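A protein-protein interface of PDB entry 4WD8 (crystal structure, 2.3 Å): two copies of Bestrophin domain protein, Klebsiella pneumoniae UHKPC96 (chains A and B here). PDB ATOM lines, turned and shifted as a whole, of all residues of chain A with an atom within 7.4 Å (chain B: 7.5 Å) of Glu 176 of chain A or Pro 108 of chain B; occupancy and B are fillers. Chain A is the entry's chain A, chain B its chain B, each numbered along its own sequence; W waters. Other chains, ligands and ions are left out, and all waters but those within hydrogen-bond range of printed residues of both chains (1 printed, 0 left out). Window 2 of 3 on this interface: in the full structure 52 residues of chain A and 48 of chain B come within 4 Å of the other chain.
Among the printed residues, pairs that only touch across the chains: Asn 169 of chain A with Pro 294 of chain B (3.8 Å), Glu 176 of chain A with Pro 108 of chain B (3.7 Å), Tyr 185 of chain A with Asn 105 of chain B (3.6 Å) and Tyr 185 of chain A with Ile 106 of chain B (3.5 Å).
The side-chain carboxylate (OD1) of Asp 182 of chain A is in salt-bridge range of the guanidinium group (NH2) of Arg 175 of chain A, at 2.9 Å.
Water W1 lies within hydrogen-bond range of NE of Arg 175 of chain A, O of Gly 172 of chain A and O of Asn 105 of chain B.
No position is printed for both chains.
Printed residues of chain B within 4 Å of Asn 169 of chain A: Asn 105 and Pro 294. Ile 171 of chain A touches none of the printed residues of chain B. Glu 176 of chain A touches just one residue of chain B: Pro 108 (3.7 Å). Printed residues of chain B within 4 Å of Tyr 185 of chain A: Asn 105 and Ile 106. Of chain A, only Glu 176 comes within 4 Å of Pro 108 of chain B.
The side-chain amide nitrogen of Asn 169 of chain A sits close to the side-chain amide nitrogen of Asn 105 of chain B. The backbone carbonyl oxygen of Ile 106 of chain B lies within hydrogen-bond range of the guanidinium group of Arg 175 of chain A (3.5 Å).
Along chain A the printed residues that touch a printed residue of chain B span positions 169 to 185. Of the 13 printed residues of chain B, 4 touch a printed residue of chain A. Hydrophobic or aromatic side chains of chain B within 4 Å of the printed part of chain A: Ile 106 and Pro 108. Among the printed residues, 6 pairs touch across the chains. Among the printed residues, no Asp or Glu carboxylate lies within 4 Å of a Lys or Arg side-chain nitrogen of the other chain.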
ATOM      1  N   ASN A 169     -16.569 -16.487  11.022  1.00  0.00           N
ATOM      2  CA  ASN A 169     -17.532 -15.715  11.806  1.00  0.00           C
ATOM      3  C   ASN A 169     -18.416 -16.583  12.699  1.00  0.00           C
ATOM      4  O   ASN A 169     -18.724 -16.202  13.830  1.00  0.00           O
ATOM      5  CB  ASN A 169     -18.416 -14.827  10.924  1.00  0.00           C
ATOM      6  CG  ASN A 169     -17.712 -13.561  10.479  1.00  0.00           C
ATOM      7  OD1 ASN A 169     -18.045 -12.983   9.442  1.00  0.00           O
ATOM      8  ND2 ASN A 169     -16.709 -13.142  11.241  1.00  0.00           N
ATOM      9  N   GLU A 170     -18.830 -17.739  12.187  1.00  0.00           N
ATOM     10  CA  GLU A 170     -19.637 -18.669  12.971  1.00  0.00           C
ATOM     11  C   GLU A 170     -18.857 -19.098  14.210  1.00  0.00           C
ATOM     12  O   GLU A 170     -19.387 -19.110  15.321  1.00  0.00           O
ATOM     13  CB  GLU A 170     -20.038 -19.885  12.141  1.00  0.00           C
ATOM     14  CG  GLU A 170     -20.962 -19.546  10.987  1.00  0.00           C
ATOM     15  CD  GLU A 170     -22.317 -19.032  11.439  1.00  0.00           C
ATOM     16  OE1 GLU A 170     -22.788 -19.450  12.517  1.00  0.00           O
ATOM     17  OE2 GLU A 170     -22.909 -18.203  10.714  1.00  0.00           O
ATOM     18  N   ILE A 171     -17.595 -19.457  14.003  1.00  0.00           N
ATOM     19  CA  ILE A 171     -16.706 -19.852  15.089  1.00  0.00           C
ATOM     20  C   ILE A 171     -16.445 -18.661  16.003  1.00  0.00           C
ATOM     21  O   ILE A 171     -16.388 -18.802  17.227  1.00  0.00           O
ATOM     22  CB  ILE A 171     -15.381 -20.401  14.546  1.00  0.00           C
ATOM     23  CG1 ILE A 171     -15.653 -21.576  13.621  1.00  0.00           C
ATOM     24  CG2 ILE A 171     -14.515 -20.900  15.671  1.00  0.00           C
ATOM     25  CD1 ILE A 171     -16.209 -22.763  14.352  1.00  0.00           C
ATOM     26  N   GLY A 172     -16.295 -17.490  15.396  1.00  0.00           N
ATOM     27  CA  GLY A 172     -16.053 -16.268  16.140  1.00  0.00           C
ATOM     28  C   GLY A 172     -17.192 -15.900  17.074  1.00  0.00           C
ATOM     29  O   GLY A 172     -16.952 -15.385  18.165  1.00  0.00           O
ATOM     30  N   GLN A 173     -18.426 -16.161  16.651  1.00  0.00           N
ATOM     31  CA  GLN A 173     -19.593 -15.867  17.481  1.00  0.00           C
ATOM     32  C   GLN A 173     -19.674 -16.808  18.676  1.00  0.00           C
ATOM     33  O   GLN A 173     -20.046 -16.397  19.773  1.00  0.00           O
ATOM     34  CB  GLN A 173     -20.890 -15.934  16.668  1.00  0.00           C
ATOM     35  CG  GLN A 173     -21.075 -14.780  15.699  1.00  0.00           C
ATOM     36  CD  GLN A 173     -22.361 -14.889  14.893  1.00  0.00           C
ATOM     37  OE1 GLN A 173     -22.917 -15.978  14.730  1.00  0.00           O
ATOM     38  NE2 GLN A 173     -22.843 -13.757  14.388  1.00  0.00           N
ATOM     39  N   LEU A 174     -19.320 -18.069  18.460  1.00  0.00           N
ATOM     40  CA  LEU A 174     -19.270 -19.042  19.544  1.00  0.00           C
ATOM     41  C   LEU A 174     -18.242 -18.616  20.588  1.00  0.00           C
ATOM     42  O   LEU A 174     -18.443 -18.823  21.783  1.00  0.00           O
ATOM     43  CB  LEU A 174     -18.940 -20.431  18.991  1.00  0.00           C
ATOM     44  CG  LEU A 174     -20.056 -21.058  18.146  1.00  0.00           C
ATOM     45  CD1 LEU A 174     -19.562 -22.272  17.367  1.00  0.00           C
ATOM     46  CD2 LEU A 174     -21.212 -21.449  19.056  1.00  0.00           C
ATOM     47  N   ARG A 175     -17.154 -17.993  20.137  1.00  0.00           N
ATOM     48  CA  ARG A 175     -16.128 -17.513  21.055  1.00  0.00           C
ATOM     49  C   ARG A 175     -16.653 -16.325  21.858  1.00  0.00           C
ATOM     50  O   ARG A 175     -16.491 -16.263  23.078  1.00  0.00           O
ATOM     51  CB  ARG A 175     -14.865 -17.103  20.297  1.00  0.00           C
ATOM     52  CG  ARG A 175     -13.655 -16.921  21.205  1.00  0.00           C
ATOM     53  CD  ARG A 175     -12.497 -16.243  20.490  1.00  0.00           C
ATOM     54  NE  ARG A 175     -12.844 -14.878  20.109  1.00  0.00           N
ATOM     55  CZ  ARG A 175     -12.608 -13.809  20.863  1.00  0.00           C
ATOM     56  NH1 ARG A 175     -12.966 -12.605  20.438  1.00  0.00           N
ATOM     57  NH2 ARG A 175     -12.011 -13.942  22.035  1.00  0.00           N
ATOM     58  N   GLU A 176     -17.289 -15.388  21.164  1.00  0.00           N
ATOM     59  CA  GLU A 176     -17.829 -14.191  21.797  1.00  0.00           C
ATOM     60  C   GLU A 176     -18.955 -14.522  22.776  1.00  0.00           C
ATOM     61  O   GLU A 176     -19.130 -13.840  23.785  1.00  0.00           O
ATOM     62  CB  GLU A 176     -18.312 -13.207  20.729  1.00  0.00           C
ATOM     63  CG  GLU A 176     -17.179 -12.671  19.857  1.00  0.00           C
ATOM     64  CD  GLU A 176     -17.647 -11.702  18.783  1.00  0.00           C
ATOM     65  OE1 GLU A 176     -18.870 -11.460  18.680  1.00  0.00           O
ATOM     66  OE2 GLU A 176     -16.788 -11.198  18.024  1.00  0.00           O
ATOM     67  N   ALA A 177     -19.708 -15.577  22.480  1.00  0.00           N
ATOM     68  CA  ALA A 177     -20.804 -16.002  23.347  1.00  0.00           C
ATOM     69  C   ALA A 177     -20.310 -16.818  24.538  1.00  0.00           C
ATOM     70  O   ALA A 177     -21.087 -17.164  25.427  1.00  0.00           O
ATOM     71  CB  ALA A 177     -21.827 -16.794  22.555  1.00  0.00           C
ATOM     72  N   GLY A 178     -19.016 -17.121  24.550  1.00  0.00           N
ATOM     73  CA  GLY A 178     -18.410 -17.858  25.642  1.00  0.00           C
ATOM     74  C   GLY A 178     -18.534 -19.367  25.527  1.00  0.00           C
ATOM     75  O   GLY A 178     -18.141 -20.092  26.440  1.00  0.00           O
ATOM     76  N   LYS A 179     -19.060 -19.853  24.408  1.00  0.00           N
ATOM     77  CA  LYS A 179     -19.195 -21.297  24.224  1.00  0.00           C
ATOM     78  C   LYS A 179     -17.861 -21.918  23.833  1.00  0.00           C
ATOM     79  O   LYS A 179     -17.573 -23.066  24.167  1.00  0.00           O
ATOM     80  CB  LYS A 179     -20.303 -21.630  23.222  1.00  0.00           C
ATOM     81  CG  LYS A 179     -21.679 -21.199  23.724  1.00  0.00           C
ATOM     82  CD  LYS A 179     -22.792 -21.507  22.744  1.00  0.00           C
ATOM     83  CE  LYS A 179     -24.138 -21.066  23.314  1.00  0.00           C
ATOM     84  NZ  LYS A 179     -25.262 -21.261  22.352  1.00  0.00           N
ATOM     85  N   LEU A 180     -17.039 -21.140  23.146  1.00  0.00           N
ATOM     86  CA  LEU A 180     -15.667 -21.536  22.913  1.00  0.00           C
ATOM     87  C   LEU A 180     -14.780 -20.604  23.716  1.00  0.00           C
ATOM     88  O   LEU A 180     -15.010 -19.399  23.753  1.00  0.00           O
ATOM     89  CB  LEU A 180     -15.314 -21.424  21.427  1.00  0.00           C
ATOM     90  CG  LEU A 180     -15.974 -22.428  20.483  1.00  0.00           C
ATOM     91  CD1 LEU A 180     -15.626 -22.118  19.026  1.00  0.00           C
ATOM     92  CD2 LEU A 180     -15.556 -23.845  20.853  1.00  0.00           C
ATOM     93  N   ASP A 182     -10.762 -19.150  24.186  1.00  0.00           N
ATOM     94  CA  ASP A 182      -9.707 -18.823  23.233  1.00  0.00           C
ATOM     95  C   ASP A 182      -8.908 -20.064  22.795  1.00  0.00           C
ATOM     96  O   ASP A 182      -8.496 -20.161  21.639  1.00  0.00           O
ATOM     97  CB  ASP A 182      -8.790 -17.728  23.788  1.00  0.00           C
ATOM     98  CG  ASP A 182      -9.473 -16.363  23.840  1.00  0.00           C
ATOM     99  OD1 ASP A 182     -10.547 -16.202  23.225  1.00  0.00           O
ATOM    100  OD2 ASP A 182      -8.927 -15.442  24.478  1.00  0.00           O
ATOM    101  N   TYR A 185     -11.261 -22.169  20.545  1.00  0.00           N
ATOM    102  CA  TYR A 185     -11.391 -21.360  19.334  1.00  0.00           C
ATOM    103  C   TYR A 185     -10.161 -21.559  18.454  1.00  0.00           C
ATOM    104  O   TYR A 185     -10.274 -21.768  17.246  1.00  0.00           O
ATOM    105  CB  TYR A 185     -11.563 -19.865  19.650  1.00  0.00           C
ATOM    106  CG  TYR A 185     -11.463 -19.016  18.408  1.00  0.00           C
ATOM    107  CD1 TYR A 185     -12.576 -18.811  17.602  1.00  0.00           C
ATOM    108  CD2 TYR A 185     -10.254 -18.439  18.020  1.00  0.00           C
ATOM    109  CE1 TYR A 185     -12.496 -18.055  16.443  1.00  0.00           C
ATOM    110  CE2 TYR A 185     -10.162 -17.685  16.853  1.00  0.00           C
ATOM    111  CZ  TYR A 185     -11.291 -17.496  16.076  1.00  0.00           C
ATOM    112  OH  TYR A 185     -11.222 -16.750  14.920  1.00  0.00           O
ATOM    113  N   GLN B 102      -8.493 -13.569  10.486  1.00  0.00           N
ATOM    114  CA  GLN B 102      -8.436 -13.639  11.940  1.00  0.00           C
ATOM    115  C   GLN B 102      -8.793 -12.294  12.577  1.00  0.00           C
ATOM    116  O   GLN B 102      -9.545 -12.242  13.554  1.00  0.00           O
ATOM    117  CB  GLN B 102      -7.057 -14.108  12.401  1.00  0.00           C
ATOM    118  CG  GLN B 102      -6.781 -15.581  12.121  1.00  0.00           C
ATOM    119  CD  GLN B 102      -5.333 -15.970  12.369  1.00  0.00           C
ATOM    120  OE1 GLN B 102      -4.424 -15.148  12.239  1.00  0.00           O
ATOM    121  NE2 GLN B 102      -5.113 -17.224  12.734  1.00  0.00           N
ATOM    122  N   LEU B 103      -8.259 -11.209  12.021  1.00  0.00           N
ATOM    123  CA  LEU B 103      -8.568  -9.867  12.513  1.00  0.00           C
ATOM    124  C   LEU B 103     -10.060  -9.546  12.395  1.00  0.00           C
ATOM    125  O   LEU B 103     -10.640  -8.903  13.274  1.00  0.00           O
ATOM    126  CB  LEU B 103      -7.760  -8.821  11.755  1.00  0.00           C
ATOM    127  CG  LEU B 103      -6.303  -8.666  12.180  1.00  0.00           C
ATOM    128  CD1 LEU B 103      -5.549  -7.930  11.085  1.00  0.00           C
ATOM    129  CD2 LEU B 103      -6.172  -7.958  13.529  1.00  0.00           C
ATOM    130  N   ARG B 104     -10.670  -9.975  11.292  1.00  0.00           N
ATOM    131  CA  ARG B 104     -12.099  -9.776  11.076  1.00  0.00           C
ATOM    132  C   ARG B 104     -12.937 -10.669  12.001  1.00  0.00           C
ATOM    133  O   ARG B 104     -13.947 -10.221  12.549  1.00  0.00           O
ATOM    134  CB  ARG B 104     -12.465  -9.994   9.598  1.00  0.00           C
ATOM    135  CG  ARG B 104     -12.040  -8.835   8.680  1.00  0.00           C
ATOM    136  CD  ARG B 104     -12.078  -9.187   7.189  1.00  0.00           C
ATOM    137  NE  ARG B 104     -11.933  -7.999   6.335  1.00  0.00           N
ATOM    138  CZ  ARG B 104     -11.798  -8.019   5.004  1.00  0.00           C
ATOM    139  NH1 ARG B 104     -11.674  -6.881   4.324  1.00  0.00           N
ATOM    140  NH2 ARG B 104     -11.775  -9.172   4.346  1.00  0.00           N
ATOM    141  N   ASN B 105     -12.521 -11.923  12.173  1.00  0.00           N
ATOM    142  CA  ASN B 105     -13.247 -12.862  13.030  1.00  0.00           C
ATOM    143  C   ASN B 105     -13.150 -12.547  14.528  1.00  0.00           C
ATOM    144  O   ASN B 105     -14.109 -12.733  15.274  1.00  0.00           O
ATOM    145  CB  ASN B 105     -12.761 -14.303  12.804  1.00  0.00           C
ATOM    146  CG  ASN B 105     -13.043 -14.823  11.393  1.00  0.00           C
ATOM    147  OD1 ASN B 105     -12.336 -15.703  10.897  1.00  0.00           O
ATOM    148  ND2 ASN B 105     -14.097 -14.314  10.765  1.00  0.00           N
ATOM    149  N   ILE B 106     -11.980 -12.093  14.964  1.00  0.00           N
ATOM    150  CA  ILE B 106     -11.698 -11.906  16.383  1.00  0.00           C
ATOM    151  C   ILE B 106     -12.011 -10.480  16.831  1.00  0.00           C
ATOM    152  O   ILE B 106     -12.514 -10.259  17.933  1.00  0.00           O
ATOM    153  CB  ILE B 106     -10.231 -12.296  16.720  1.00  0.00           C
ATOM    154  CG1 ILE B 106      -9.984 -13.766  16.383  1.00  0.00           C
ATOM    155  CG2 ILE B 106      -9.914 -12.052  18.184  1.00  0.00           C
ATOM    156  CD1 ILE B 106      -8.520 -14.185  16.480  1.00  0.00           C
ATOM    157  N   LEU B 107     -11.734  -9.514  15.958  1.00  0.00           N
ATOM    158  CA  LEU B 107     -12.001  -8.110  16.257  1.00  0.00           C
ATOM    159  C   LEU B 107     -12.807  -7.467  15.132  1.00  0.00           C
ATOM    160  O   LEU B 107     -12.318  -6.553  14.467  1.00  0.00           O
ATOM    161  CB  LEU B 107     -10.680  -7.361  16.439  1.00  0.00           C
ATOM    162  CG  LEU B 107      -9.763  -7.844  17.568  1.00  0.00           C
ATOM    163  CD1 LEU B 107      -8.397  -7.175  17.486  1.00  0.00           C
ATOM    164  CD2 LEU B 107     -10.404  -7.583  18.933  1.00  0.00           C
ATOM    165  N   PRO B 108     -14.054  -7.928  14.928  1.00  0.00           N
ATOM    166  CA  PRO B 108     -14.847  -7.514  13.763  1.00  0.00           C
ATOM    167  C   PRO B 108     -15.101  -6.019  13.635  1.00  0.00           C
ATOM    168  O   PRO B 108     -15.321  -5.549  12.518  1.00  0.00           O
ATOM    169  CB  PRO B 108     -16.184  -8.246  13.970  1.00  0.00           C
ATOM    170  CG  PRO B 108     -16.235  -8.557  15.428  1.00  0.00           C
ATOM    171  CD  PRO B 108     -14.813  -8.828  15.814  1.00  0.00           C
ATOM    172  N   ALA B 109     -15.052  -5.288  14.744  1.00  0.00           N
ATOM    173  CA  ALA B 109     -15.378  -3.864  14.737  1.00  0.00           C
ATOM    174  C   ALA B 109     -14.164  -2.931  14.648  1.00  0.00           C
ATOM    175  O   ALA B 109     -14.321  -1.717  14.530  1.00  0.00           O
ATOM    176  CB  ALA B 109     -16.240  -3.514  15.944  1.00  0.00           C
ATOM    177  N   GLU B 110     -12.958  -3.488  14.708  1.00  0.00           N
ATOM    178  CA  GLU B 110     -11.747  -2.663  14.717  1.00  0.00           C
ATOM    179  C   GLU B 110     -11.277  -2.303  13.308  1.00  0.00           C
ATOM    180  O   GLU B 110     -10.187  -2.694  12.894  1.00  0.00           O
ATOM    181  CB  GLU B 110     -10.615  -3.371  15.470  1.00  0.00           C
ATOM    182  CG  GLU B 110     -10.894  -3.650  16.930  1.00  0.00           C
ATOM    183  CD  GLU B 110     -10.916  -2.383  17.773  1.00  0.00           C
ATOM    184  OE1 GLU B 110     -10.217  -1.407  17.415  1.00  0.00           O
ATOM    185  OE2 GLU B 110     -11.626  -2.368  18.800  1.00  0.00           O
ATOM    186  N   HIS B 111     -12.094  -1.545  12.581  1.00  0.00           N
ATOM    187  CA  HIS B 111     -11.820  -1.272  11.173  1.00  0.00           C
ATOM    188  C   HIS B 111     -10.592  -0.387  10.939  1.00  0.00           C
ATOM    189  O   HIS B 111      -9.898  -0.548   9.934  1.00  0.00           O
ATOM    190  CB  HIS B 111     -13.050  -0.705  10.454  1.00  0.00           C
ATOM    191  CG  HIS B 111     -14.267  -1.573  10.556  1.00  0.00           C
ATOM    192  ND1 HIS B 111     -14.328  -2.843  10.017  1.00  0.00           N
ATOM    193  CD2 HIS B 111     -15.484  -1.336  11.097  1.00  0.00           C
ATOM    194  CE1 HIS B 111     -15.523  -3.357  10.246  1.00  0.00           C
ATOM    195  NE2 HIS B 111     -16.246  -2.462  10.896  1.00  0.00           N
ATOM    196  N   HIS B 114      -7.833  -2.787  11.125  1.00  0.00           N
ATOM    197  CA  HIS B 114      -7.864  -3.594   9.905  1.00  0.00           C
ATOM    198  C   HIS B 114      -7.143  -2.878   8.772  1.00  0.00           C
ATOM    199  O   HIS B 114      -6.304  -3.469   8.091  1.00  0.00           O
ATOM    200  CB  HIS B 114      -9.301  -3.885   9.467  1.00  0.00           C
ATOM    201  CG  HIS B 114     -10.091  -4.675  10.460  1.00  0.00           C
ATOM    202  ND1 HIS B 114     -11.468  -4.728  10.440  1.00  0.00           N
ATOM    203  CD2 HIS B 114      -9.696  -5.448  11.499  1.00  0.00           C
ATOM    204  CE1 HIS B 114     -11.887  -5.501  11.426  1.00  0.00           C
ATOM    205  NE2 HIS B 114     -10.832  -5.950  12.084  1.00  0.00           N
ATOM    206  N   HIS B 293     -16.163  -6.128   5.005  1.00  0.00           N
ATOM    207  CA  HIS B 293     -16.458  -7.510   5.359  1.00  0.00           C
ATOM    208  C   HIS B 293     -17.782  -7.637   6.103  1.00  0.00           C
ATOM    209  O   HIS B 293     -18.238  -6.702   6.756  1.00  0.00           O
ATOM    210  CB  HIS B 293     -15.331  -8.079   6.231  1.00  0.00           C
ATOM    211  CG  HIS B 293     -14.964  -7.217   7.399  1.00  0.00           C
ATOM    212  ND1 HIS B 293     -15.320  -7.528   8.696  1.00  0.00           N
ATOM    213  CD2 HIS B 293     -14.266  -6.056   7.472  1.00  0.00           C
ATOM    214  CE1 HIS B 293     -14.856  -6.600   9.512  1.00  0.00           C
ATOM    215  NE2 HIS B 293     -14.211  -5.694   8.795  1.00  0.00           N
ATOM    216  N   PRO B 294     -18.416  -8.803   5.980  1.00  0.00           N
ATOM    217  CA  PRO B 294     -19.593  -9.140   6.781  1.00  0.00           C
ATOM    218  C   PRO B 294     -19.213  -9.358   8.240  1.00  0.00           C
ATOM    219  O   PRO B 294     -20.062  -9.783   9.022  1.00  0.00           O
ATOM    220  CB  PRO B 294     -20.040 -10.466   6.180  1.00  0.00           C
ATOM    221  CG  PRO B 294     -19.453 -10.476   4.791  1.00  0.00           C
ATOM    222  CD  PRO B 294     -18.138  -9.823   4.955  1.00  0.00           C
HETATM  223  O   HOH W   1     -14.378 -13.738  18.324  1.00  0.00           O
